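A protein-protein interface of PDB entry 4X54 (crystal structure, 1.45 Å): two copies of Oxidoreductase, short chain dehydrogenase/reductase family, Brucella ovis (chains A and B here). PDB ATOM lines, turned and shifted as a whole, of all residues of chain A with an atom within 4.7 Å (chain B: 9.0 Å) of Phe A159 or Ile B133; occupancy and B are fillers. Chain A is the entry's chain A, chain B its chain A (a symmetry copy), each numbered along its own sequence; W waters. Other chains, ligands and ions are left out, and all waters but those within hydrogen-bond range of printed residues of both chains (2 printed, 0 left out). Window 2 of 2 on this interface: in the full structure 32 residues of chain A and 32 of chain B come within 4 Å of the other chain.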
ATOM      1  N   ALA A 155      16.023  20.101  26.146  1.00  0.00           N
ATOM      2  CA  ALA A 155      15.355  21.339  26.538  1.00  0.00           C
ATOM      3  C   ALA A 155      14.108  21.070  27.359  1.00  0.00           C
ATOM      4  O   ALA A 155      13.886  21.731  28.398  1.00  0.00           O
ATOM      5  CB  ALA A 155      14.995  22.171  25.274  1.00  0.00           C
ATOM      6  N   ARG A 156      13.277  20.115  26.959  1.00  0.00           N
ATOM      7  CA  ARG A 156      12.066  19.885  27.740  1.00  0.00           C
ATOM      8  C   ARG A 156      12.385  19.096  29.021  1.00  0.00           C
ATOM      9  O   ARG A 156      11.730  19.274  30.057  1.00  0.00           O
ATOM     10  CB  ARG A 156      10.961  19.236  26.883  1.00  0.00           C
ATOM     11  CG  ARG A 156      11.174  17.800  26.389  1.00  0.00           C
ATOM     12  CD  ARG A 156      10.208  17.565  25.210  1.00  0.00           C
ATOM     13  NE  ARG A 156      10.200  16.148  24.814  1.00  0.00           N
ATOM     14  CZ  ARG A 156       9.388  15.719  23.879  1.00  0.00           C
ATOM     15  NH1 ARG A 156       8.587  16.586  23.284  1.00  0.00           N
ATOM     16  NH2 ARG A 156       9.364  14.431  23.559  1.00  0.00           N
ATOM     17  N   GLY A 157      13.435  18.237  28.983  1.00  0.00           N
ATOM     18  CA  GLY A 157      13.856  17.540  30.188  1.00  0.00           C
ATOM     19  C   GLY A 157      14.378  18.460  31.281  1.00  0.00           C
ATOM     20  O   GLY A 157      14.241  18.157  32.459  1.00  0.00           O
ATOM     21  N   LEU A 158      15.022  19.543  30.837  1.00  0.00           N
ATOM     22  CA  LEU A 158      15.625  20.528  31.721  1.00  0.00           C
ATOM     23  C   LEU A 158      14.742  21.786  31.828  1.00  0.00           C
ATOM     24  O   LEU A 158      15.227  22.848  32.246  1.00  0.00           O
ATOM     25  CB  LEU A 158      17.027  20.890  31.206  1.00  0.00           C
ATOM     26  CG  LEU A 158      17.947  19.670  31.216  1.00  0.00           C
ATOM     27  CD1 LEU A 158      19.263  20.018  30.434  1.00  0.00           C
ATOM     28  CD2 LEU A 158      18.295  19.342  32.654  1.00  0.00           C
ATOM     29  N   PHE A 159      13.470  21.627  31.482  1.00  0.00           N
ATOM     30  CA  PHE A 159      12.577  22.778  31.382  1.00  0.00           C
ATOM     31  C   PHE A 159      12.423  23.513  32.706  1.00  0.00           C
ATOM     32  O   PHE A 159      12.451  24.757  32.731  1.00  0.00           O
ATOM     33  CB  PHE A 159      11.190  22.312  30.899  1.00  0.00           C
ATOM     34  CG  PHE A 159      10.305  23.436  30.425  1.00  0.00           C
ATOM     35  CD1 PHE A 159       9.572  24.155  31.300  1.00  0.00           C
ATOM     36  CD2 PHE A 159      10.273  23.757  29.073  1.00  0.00           C
ATOM     37  CE1 PHE A 159       8.749  25.233  30.838  1.00  0.00           C
ATOM     38  CE2 PHE A 159       9.475  24.790  28.594  1.00  0.00           C
ATOM     39  CZ  PHE A 159       8.730  25.533  29.510  1.00  0.00           C
ATOM     40  N   LYS A 160      12.323  22.780  33.821  1.00  0.00           N
ATOM     41  CA  LYS A 160      12.082  23.444  35.127  1.00  0.00           C
ATOM     42  C   LYS A 160      13.272  24.378  35.459  1.00  0.00           C
ATOM     43  O   LYS A 160      13.108  25.507  35.946  1.00  0.00           O
ATOM     44  CB  LYS A 160      11.889  22.394  36.203  1.00  0.00           C
ATOM     45  N   GLU A 161      14.478  23.887  35.164  1.00  0.00           N
ATOM     46  CA  GLU A 161      15.661  24.656  35.505  1.00  0.00           C
ATOM     47  C   GLU A 161      15.877  25.824  34.527  1.00  0.00           C
ATOM     48  O   GLU A 161      16.310  26.911  34.980  1.00  0.00           O
ATOM     49  CB  GLU A 161      16.913  23.724  35.528  1.00  0.00           C
ATOM     50  CG  GLU A 161      16.942  22.698  36.674  1.00  0.00           C
ATOM     51  CD  GLU A 161      16.041  21.455  36.485  1.00  0.00           C
ATOM     52  OE1 GLU A 161      15.462  21.229  35.382  1.00  0.00           O
ATOM     53  OE2 GLU A 161      16.002  20.712  37.534  1.00  0.00           O
ATOM     54  N   LEU A 162      15.592  25.625  33.227  1.00  0.00           N
ATOM     55  CA  LEU A 162      15.642  26.749  32.285  1.00  0.00           C
ATOM     56  C   LEU A 162      14.605  27.825  32.672  1.00  0.00           C
ATOM     57  O   LEU A 162      14.873  29.039  32.601  1.00  0.00           O
ATOM     58  CB  LEU A 162      15.363  26.245  30.867  1.00  0.00           C
ATOM     59  CG  LEU A 162      16.503  25.437  30.238  1.00  0.00           C
ATOM     60  CD1 LEU A 162      15.917  24.681  29.038  1.00  0.00           C
ATOM     61  CD2 LEU A 162      17.623  26.399  29.821  1.00  0.00           C
ATOM     62  N   GLU A 163      13.412  27.376  33.084  1.00  0.00           N
ATOM     63  CA  GLU A 163      12.373  28.333  33.491  1.00  0.00           C
ATOM     64  C   GLU A 163      12.768  29.087  34.762  1.00  0.00           C
ATOM     65  O   GLU A 163      12.587  30.300  34.843  1.00  0.00           O
ATOM     66  CB  GLU A 163      11.038  27.612  33.675  1.00  0.00           C
ATOM     67  CG  GLU A 163       9.875  28.588  33.944  1.00  0.00           C
ATOM     68  CD  GLU A 163       8.627  27.853  34.334  1.00  0.00           C
ATOM     69  OE1 GLU A 163       8.747  26.809  35.023  1.00  0.00           O
ATOM     70  OE2 GLU A 163       7.536  28.324  33.977  1.00  0.00           O
ATOM     71  N   ASP A 205       7.058  28.208  21.413  1.00  0.00           N
ATOM     72  CA  ASP A 205       6.544  27.429  22.541  1.00  0.00           C
ATOM     73  C   ASP A 205       7.092  27.797  23.892  1.00  0.00           C
ATOM     74  O   ASP A 205       6.338  27.762  24.886  1.00  0.00           O
ATOM     75  CB  ASP A 205       6.851  25.964  22.304  1.00  0.00           C
ATOM     76  CG  ASP A 205       6.200  25.425  20.999  1.00  0.00           C
ATOM     77  OD1 ASP A 205       5.200  26.007  20.520  1.00  0.00           O
ATOM     78  OD2 ASP A 205       6.746  24.411  20.524  1.00  0.00           O
ATOM     79  N   PHE A 206       8.384  28.145  23.918  1.00  0.00           N
ATOM     80  CA  PHE A 206       9.093  28.434  25.171  1.00  0.00           C
ATOM     81  C   PHE A 206       8.951  29.901  25.583  1.00  0.00           C
ATOM     82  O   PHE A 206       9.123  30.221  26.754  1.00  0.00           O
ATOM     83  CB  PHE A 206      10.597  28.062  25.015  1.00  0.00           C
ATOM     84  CG  PHE A 206      10.882  26.600  25.128  1.00  0.00           C
ATOM     85  CD1 PHE A 206      10.389  25.651  24.190  1.00  0.00           C
ATOM     86  CD2 PHE A 206      11.707  26.152  26.103  1.00  0.00           C
ATOM     87  CE1 PHE A 206      10.710  24.296  24.308  1.00  0.00           C
ATOM     88  CE2 PHE A 206      12.035  24.787  26.238  1.00  0.00           C
ATOM     89  CZ  PHE A 206      11.547  23.846  25.282  1.00  0.00           C
ATOM     90  N   TYR A 209       7.021  31.091  28.619  1.00  0.00           N
ATOM     91  CA  TYR A 209       7.626  30.666  29.882  1.00  0.00           C
ATOM     92  C   TYR A 209       8.853  31.488  30.207  1.00  0.00           C
ATOM     93  O   TYR A 209       9.473  31.285  31.258  1.00  0.00           O
ATOM     94  CB  TYR A 209       7.957  29.177  29.825  1.00  0.00           C
ATOM     95  CG  TYR A 209       6.734  28.323  29.659  1.00  0.00           C
ATOM     96  CD1 TYR A 209       5.995  27.987  30.754  1.00  0.00           C
ATOM     97  CD2 TYR A 209       6.332  27.887  28.402  1.00  0.00           C
ATOM     98  CE1 TYR A 209       4.829  27.223  30.619  1.00  0.00           C
ATOM     99  CE2 TYR A 209       5.172  27.139  28.251  1.00  0.00           C
ATOM    100  CZ  TYR A 209       4.455  26.801  29.365  1.00  0.00           C
ATOM    101  OH  TYR A 209       3.311  26.043  29.215  1.00  0.00           O
ATOM    102  N   ILE A 211      11.702  31.704  28.309  1.00  0.00           N
ATOM    103  CA  ILE A 211      12.940  31.051  27.853  1.00  0.00           C
ATOM    104  C   ILE A 211      13.139  31.380  26.390  1.00  0.00           C
ATOM    105  O   ILE A 211      12.281  31.071  25.585  1.00  0.00           O
ATOM    106  CB  ILE A 211      12.843  29.517  28.020  1.00  0.00           C
ATOM    107  CG1 ILE A 211      12.684  29.145  29.519  1.00  0.00           C
ATOM    108  CG2 ILE A 211      14.146  28.847  27.485  1.00  0.00           C
ATOM    109  CD1 ILE A 211      12.062  27.718  29.704  1.00  0.00           C
ATOM    110  N   ARG B 128      -6.140  19.823  19.883  1.00  0.00           N
ATOM    111  CA  ARG B 128      -5.224  20.935  19.982  1.00  0.00           C
ATOM    112  C   ARG B 128      -3.985  20.712  19.061  1.00  0.00           C
ATOM    113  O   ARG B 128      -3.540  19.591  18.802  1.00  0.00           O
ATOM    114  CB  ARG B 128      -4.737  21.121  21.421  1.00  0.00           C
ATOM    115  CG  ARG B 128      -5.776  21.570  22.424  1.00  0.00           C
ATOM    116  CD  ARG B 128      -5.119  21.814  23.777  1.00  0.00           C
ATOM    117  NE  ARG B 128      -4.334  20.663  24.220  1.00  0.00           N
ATOM    118  CZ  ARG B 128      -3.008  20.637  24.306  1.00  0.00           C
ATOM    119  NH1 ARG B 128      -2.295  21.704  23.982  1.00  0.00           N
ATOM    120  NH2 ARG B 128      -2.401  19.536  24.734  1.00  0.00           N
ATOM    121  N   ARG B 129      -3.439  21.806  18.579  1.00  0.00           N
ATOM    122  CA  ARG B 129      -2.152  21.793  17.908  1.00  0.00           C
ATOM    123  C   ARG B 129      -1.094  21.216  18.841  1.00  0.00           C
ATOM    124  O   ARG B 129      -1.056  21.588  20.036  1.00  0.00           O
ATOM    125  CB  ARG B 129      -1.821  23.215  17.529  1.00  0.00           C
ATOM    126  CG  ARG B 129      -0.583  23.368  16.752  1.00  0.00           C
ATOM    127  CD  ARG B 129      -0.349  24.860  16.663  1.00  0.00           C
ATOM    128  NE  ARG B 129       0.798  25.061  15.806  1.00  0.00           N
ATOM    129  CZ  ARG B 129       2.052  25.032  16.263  1.00  0.00           C
ATOM    130  NH1 ARG B 129       2.288  24.870  17.545  1.00  0.00           N
ATOM    131  NH2 ARG B 129       3.053  25.210  15.426  1.00  0.00           N
ATOM    132  N   MET B 130      -0.247  20.331  18.317  1.00  0.00           N
ATOM    133  CA  MET B 130       0.755  19.638  19.142  1.00  0.00           C
ATOM    134  C   MET B 130       2.127  20.311  18.955  1.00  0.00           C
ATOM    135  O   MET B 130       2.683  20.329  17.852  1.00  0.00           O
ATOM    136  CB  MET B 130       0.827  18.178  18.726  1.00  0.00           C
ATOM    137  CG  MET B 130       1.608  17.351  19.723  1.00  0.00           C
ATOM    138  SD  MET B 130       1.907  15.657  19.137  1.00  0.00           S
ATOM    139  CE  MET B 130       0.212  15.007  19.061  1.00  0.00           C
ATOM    140  N   ASN B 131       2.615  20.896  20.048  1.00  0.00           N
ATOM    141  CA  ASN B 131       3.860  21.721  19.948  1.00  0.00           C
ATOM    142  C   ASN B 131       5.122  20.936  20.360  1.00  0.00           C
ATOM    143  O   ASN B 131       5.088  19.714  20.599  1.00  0.00           O
ATOM    144  CB  ASN B 131       3.719  23.011  20.740  1.00  0.00           C
ATOM    145  CG  ASN B 131       3.759  22.812  22.228  1.00  0.00           C
ATOM    146  OD1 ASN B 131       4.101  21.715  22.743  1.00  0.00           O
ATOM    147  ND2 ASN B 131       3.434  23.896  22.978  1.00  0.00           N
ATOM    148  N   SER B 132       6.253  21.650  20.424  1.00  0.00           N
ATOM    149  CA  SER B 132       7.526  20.959  20.618  1.00  0.00           C
ATOM    150  C   SER B 132       7.647  20.371  22.006  1.00  0.00           C
ATOM    151  O   SER B 132       8.327  19.348  22.187  1.00  0.00           O
ATOM    152  CB  SER B 132       8.670  21.912  20.346  1.00  0.00           C
ATOM    153  OG  SER B 132       8.799  22.872  21.383  1.00  0.00           O
ATOM    154  N   ILE B 133       6.978  20.949  22.985  1.00  0.00           N
ATOM    155  CA  ILE B 133       7.055  20.491  24.363  1.00  0.00           C
ATOM    156  C   ILE B 133       6.232  19.208  24.538  1.00  0.00           C
ATOM    157  O   ILE B 133       6.612  18.351  25.319  1.00  0.00           O
ATOM    158  CB  ILE B 133       6.549  21.616  25.299  1.00  0.00           C
ATOM    159  CG1 ILE B 133       7.519  22.803  25.224  1.00  0.00           C
ATOM    160  CG2 ILE B 133       6.443  21.161  26.748  1.00  0.00           C
ATOM    161  CD1 ILE B 133       6.985  24.122  25.842  1.00  0.00           C
ATOM    162  N   GLU B 134       5.106  19.127  23.817  1.00  0.00           N
ATOM    163  CA  GLU B 134       4.090  18.092  24.062  1.00  0.00           C
ATOM    164  C   GLU B 134       4.202  16.901  23.122  1.00  0.00           C
ATOM    165  O   GLU B 134       3.466  15.912  23.276  1.00  0.00           O
ATOM    166  CB  GLU B 134       2.683  18.692  23.919  1.00  0.00           C
ATOM    167  CG  GLU B 134       2.426  19.824  24.918  1.00  0.00           C
ATOM    168  CD  GLU B 134       0.968  20.283  24.858  1.00  0.00           C
ATOM    169  OE1 GLU B 134       0.716  21.493  25.022  1.00  0.00           O
ATOM    170  OE2 GLU B 134       0.087  19.428  24.623  1.00  0.00           O
ATOM    171  N   THR B 135       5.031  16.965  22.081  1.00  0.00           N
ATOM    172  CA  THR B 135       5.029  15.875  21.070  1.00  0.00           C
ATOM    173  C   THR B 135       5.798  14.671  21.582  1.00  0.00           C
ATOM    174  O   THR B 135       6.990  14.804  21.848  1.00  0.00           O
ATOM    175  CB  THR B 135       5.698  16.372  19.775  1.00  0.00           C
ATOM    176  OG1 THR B 135       4.930  17.462  19.222  1.00  0.00           O
ATOM    177  CG2 THR B 135       5.758  15.286  18.744  1.00  0.00           C
ATOM    178  N   PRO B 136       5.166  13.515  21.708  1.00  0.00           N
ATOM    179  CA  PRO B 136       5.899  12.345  22.213  1.00  0.00           C
ATOM    180  C   PRO B 136       6.806  11.786  21.137  1.00  0.00           C
ATOM    181  O   PRO B 136       6.615  11.969  19.932  1.00  0.00           O
ATOM    182  CB  PRO B 136       4.793  11.314  22.528  1.00  0.00           C
ATOM    183  CG  PRO B 136       3.473  12.073  22.523  1.00  0.00           C
ATOM    184  CD  PRO B 136       3.713  13.270  21.575  1.00  0.00           C
ATOM    185  N   MET B 137       7.822  11.073  21.567  1.00  0.00           N
ATOM    186  CA  MET B 137       8.728  10.366  20.685  1.00  0.00           C
ATOM    187  C   MET B 137       8.046   9.616  19.567  1.00  0.00           C
ATOM    188  O   MET B 137       8.511   9.643  18.401  1.00  0.00           O
ATOM    189  CB  MET B 137       9.534   9.300  21.487  1.00  0.00           C
ATOM    190  CG  MET B 137      10.620   9.887  22.356  1.00  0.00           C
ATOM    191  SD  MET B 137      11.596   8.449  22.990  1.00  0.00           S
ATOM    192  CE  MET B 137      12.354   7.731  21.564  1.00  0.00           C
ATOM    193  N   TRP B 140       6.928  12.081  16.816  1.00  0.00           N
ATOM    194  CA  TRP B 140       8.030  12.557  15.990  1.00  0.00           C
ATOM    195  C   TRP B 140       8.449  11.471  14.997  1.00  0.00           C
ATOM    196  O   TRP B 140       8.703  11.740  13.807  1.00  0.00           O
ATOM    197  CB  TRP B 140       9.266  12.869  16.866  1.00  0.00           C
ATOM    198  CG  TRP B 140       9.171  14.013  17.827  1.00  0.00           C
ATOM    199  CD1 TRP B 140       9.046  13.907  19.177  1.00  0.00           C
ATOM    200  CD2 TRP B 140       9.236  15.437  17.534  1.00  0.00           C
ATOM    201  NE1 TRP B 140       9.049  15.160  19.739  1.00  0.00           N
ATOM    202  CE2 TRP B 140       9.143  16.108  18.760  1.00  0.00           C
ATOM    203  CE3 TRP B 140       9.357  16.188  16.358  1.00  0.00           C
ATOM    204  CZ2 TRP B 140       9.165  17.488  18.875  1.00  0.00           C
ATOM    205  CZ3 TRP B 140       9.328  17.560  16.469  1.00  0.00           C
ATOM    206  CH2 TRP B 140       9.267  18.197  17.728  1.00  0.00           C
ATOM    207  N   THR B 186       4.239  21.001  15.440  1.00  0.00           N
ATOM    208  CA  THR B 186       5.671  21.090  15.295  1.00  0.00           C
ATOM    209  C   THR B 186       6.271  19.910  14.540  1.00  0.00           C
ATOM    210  O   THR B 186       7.202  20.106  13.733  1.00  0.00           O
ATOM    211  CB  THR B 186       6.298  21.209  16.677  1.00  0.00           C
ATOM    212  OG1 THR B 186       5.778  22.359  17.321  1.00  0.00           O
ATOM    213  CG2 THR B 186       7.842  21.325  16.539  1.00  0.00           C
ATOM    214  N   ALA B 187       5.769  18.691  14.732  1.00  0.00           N
ATOM    215  CA  ALA B 187       6.336  17.572  13.986  1.00  0.00           C
ATOM    216  C   ALA B 187       6.072  17.752  12.478  1.00  0.00           C
ATOM    217  O   ALA B 187       6.974  17.490  11.666  1.00  0.00           O
ATOM    218  CB  ALA B 187       5.720  16.288  14.508  1.00  0.00           C
HETATM  219  O   HOH W   1       4.805  26.078  17.972  1.00  0.00           O
HETATM  220  O   HOH W   2       2.920  26.605  21.664  1.00  0.00           O
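The guanidinium group (NH1) of Arg A156 lies within hydrogen-bond range of the backbone carbonyl oxygen (O) of Ser B132 (3.0 Å).
The backbone carbonyl oxygen of Ile B133 is in hydrogen-bond range of the guanidinium group of Arg A156 (3.3 Å).
NH1 of Arg A156 lies within hydrogen-bond range of O of Thr B135 (2.8 Å).
The side-chain carboxylate (OD2) of Asp A205 is in hydrogen-bond range of the side-chain hydroxyl (OG) of Ser B132 (2.7 Å).
The backbone carbonyl oxygen (O) of Phe A206 lies within hydrogen-bond range of the backbone NH (N) of Ile A211 (3.4 Å).
The side-chain hydroxyl (OG1) of Thr B135 lies close to the side-chain sulfur (SD) of Met B130 (3.5 Å).
The backbone NH (N) of Thr B186 sits at hydrogen-bond distance from the backbone carbonyl oxygen (O) of Met B130.
The backbone NH (N) of Ile B133 sits at hydrogen-bond distance from the side-chain amide oxygen (OD1) of Asn B131 (3.0 Å).
OD1 of Asn B131 lies within hydrogen-bond range of N of Glu B134, at 3.0 Å.
The side-chain hydroxyl (OG1) of Thr B186 lies within hydrogen-bond range of the backbone NH (N) of Ser B132 (3.2 Å).
Trp B140 touches Arg A156.
CE2 of Phe A159 touches CD1 of Ile B133, 3.8 Å away.
Asn B131 touches Asp A205 (CB to OD2, 3.3 Å).
CD1 of Ile B133 touches O of Asp A205, 3.8 Å away.
Asp A205 touches Thr B186.
Ser B132 touches Phe A206.
Phe A206 touches Ile B133.
Of chain A, only Arg A156 (3.3 Å), Phe A159 (3.8 Å), Asp A205 (3.8 Å) and Phe A206 (3.6 Å) come within 4 Å of Ile B133.
No residue of chain B comes within 4 Å of Gly A157.
Of the printed residues of chain B, Arg A156 touches Ser B132 (3.0 Å), Ile B133 (3.3 Å), Thr B135 (2.8 Å) and Trp B140 (3.8 Å).
Of the printed residues of chain A, Thr B186 touches Asp A205 (3.9 Å).
Of the printed residues of chain A, Trp B140 touches Arg A156 (3.8 Å).
Met B130 touches none of the printed residues of chain A.
Printed residues of chain B that touch a printed residue of chain A: Asn B131, Ser B132, Ile B133, Thr B135, Trp B140 and Thr B186.
Hydrophobic or aromatic side chains of chain B within 4 Å of the printed part of chain A: Ile B133 and Trp B140.
Printed residues of chain A that touch a printed residue of chain B: Arg A156, Phe A159, Asp A205 and Phe A206.
Hydrophobic or aromatic side chains of chain A that line the printed part of chain B: Phe A159 and Phe A206.
No position is printed for both chains.
Water W1 lies within hydrogen-bond range of OD1 of Asp A205 and NH1 of Arg B129.
Water W2 lies within hydrogen-bond range of OD1 of Asp A205 and ND2 of Asn B131.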
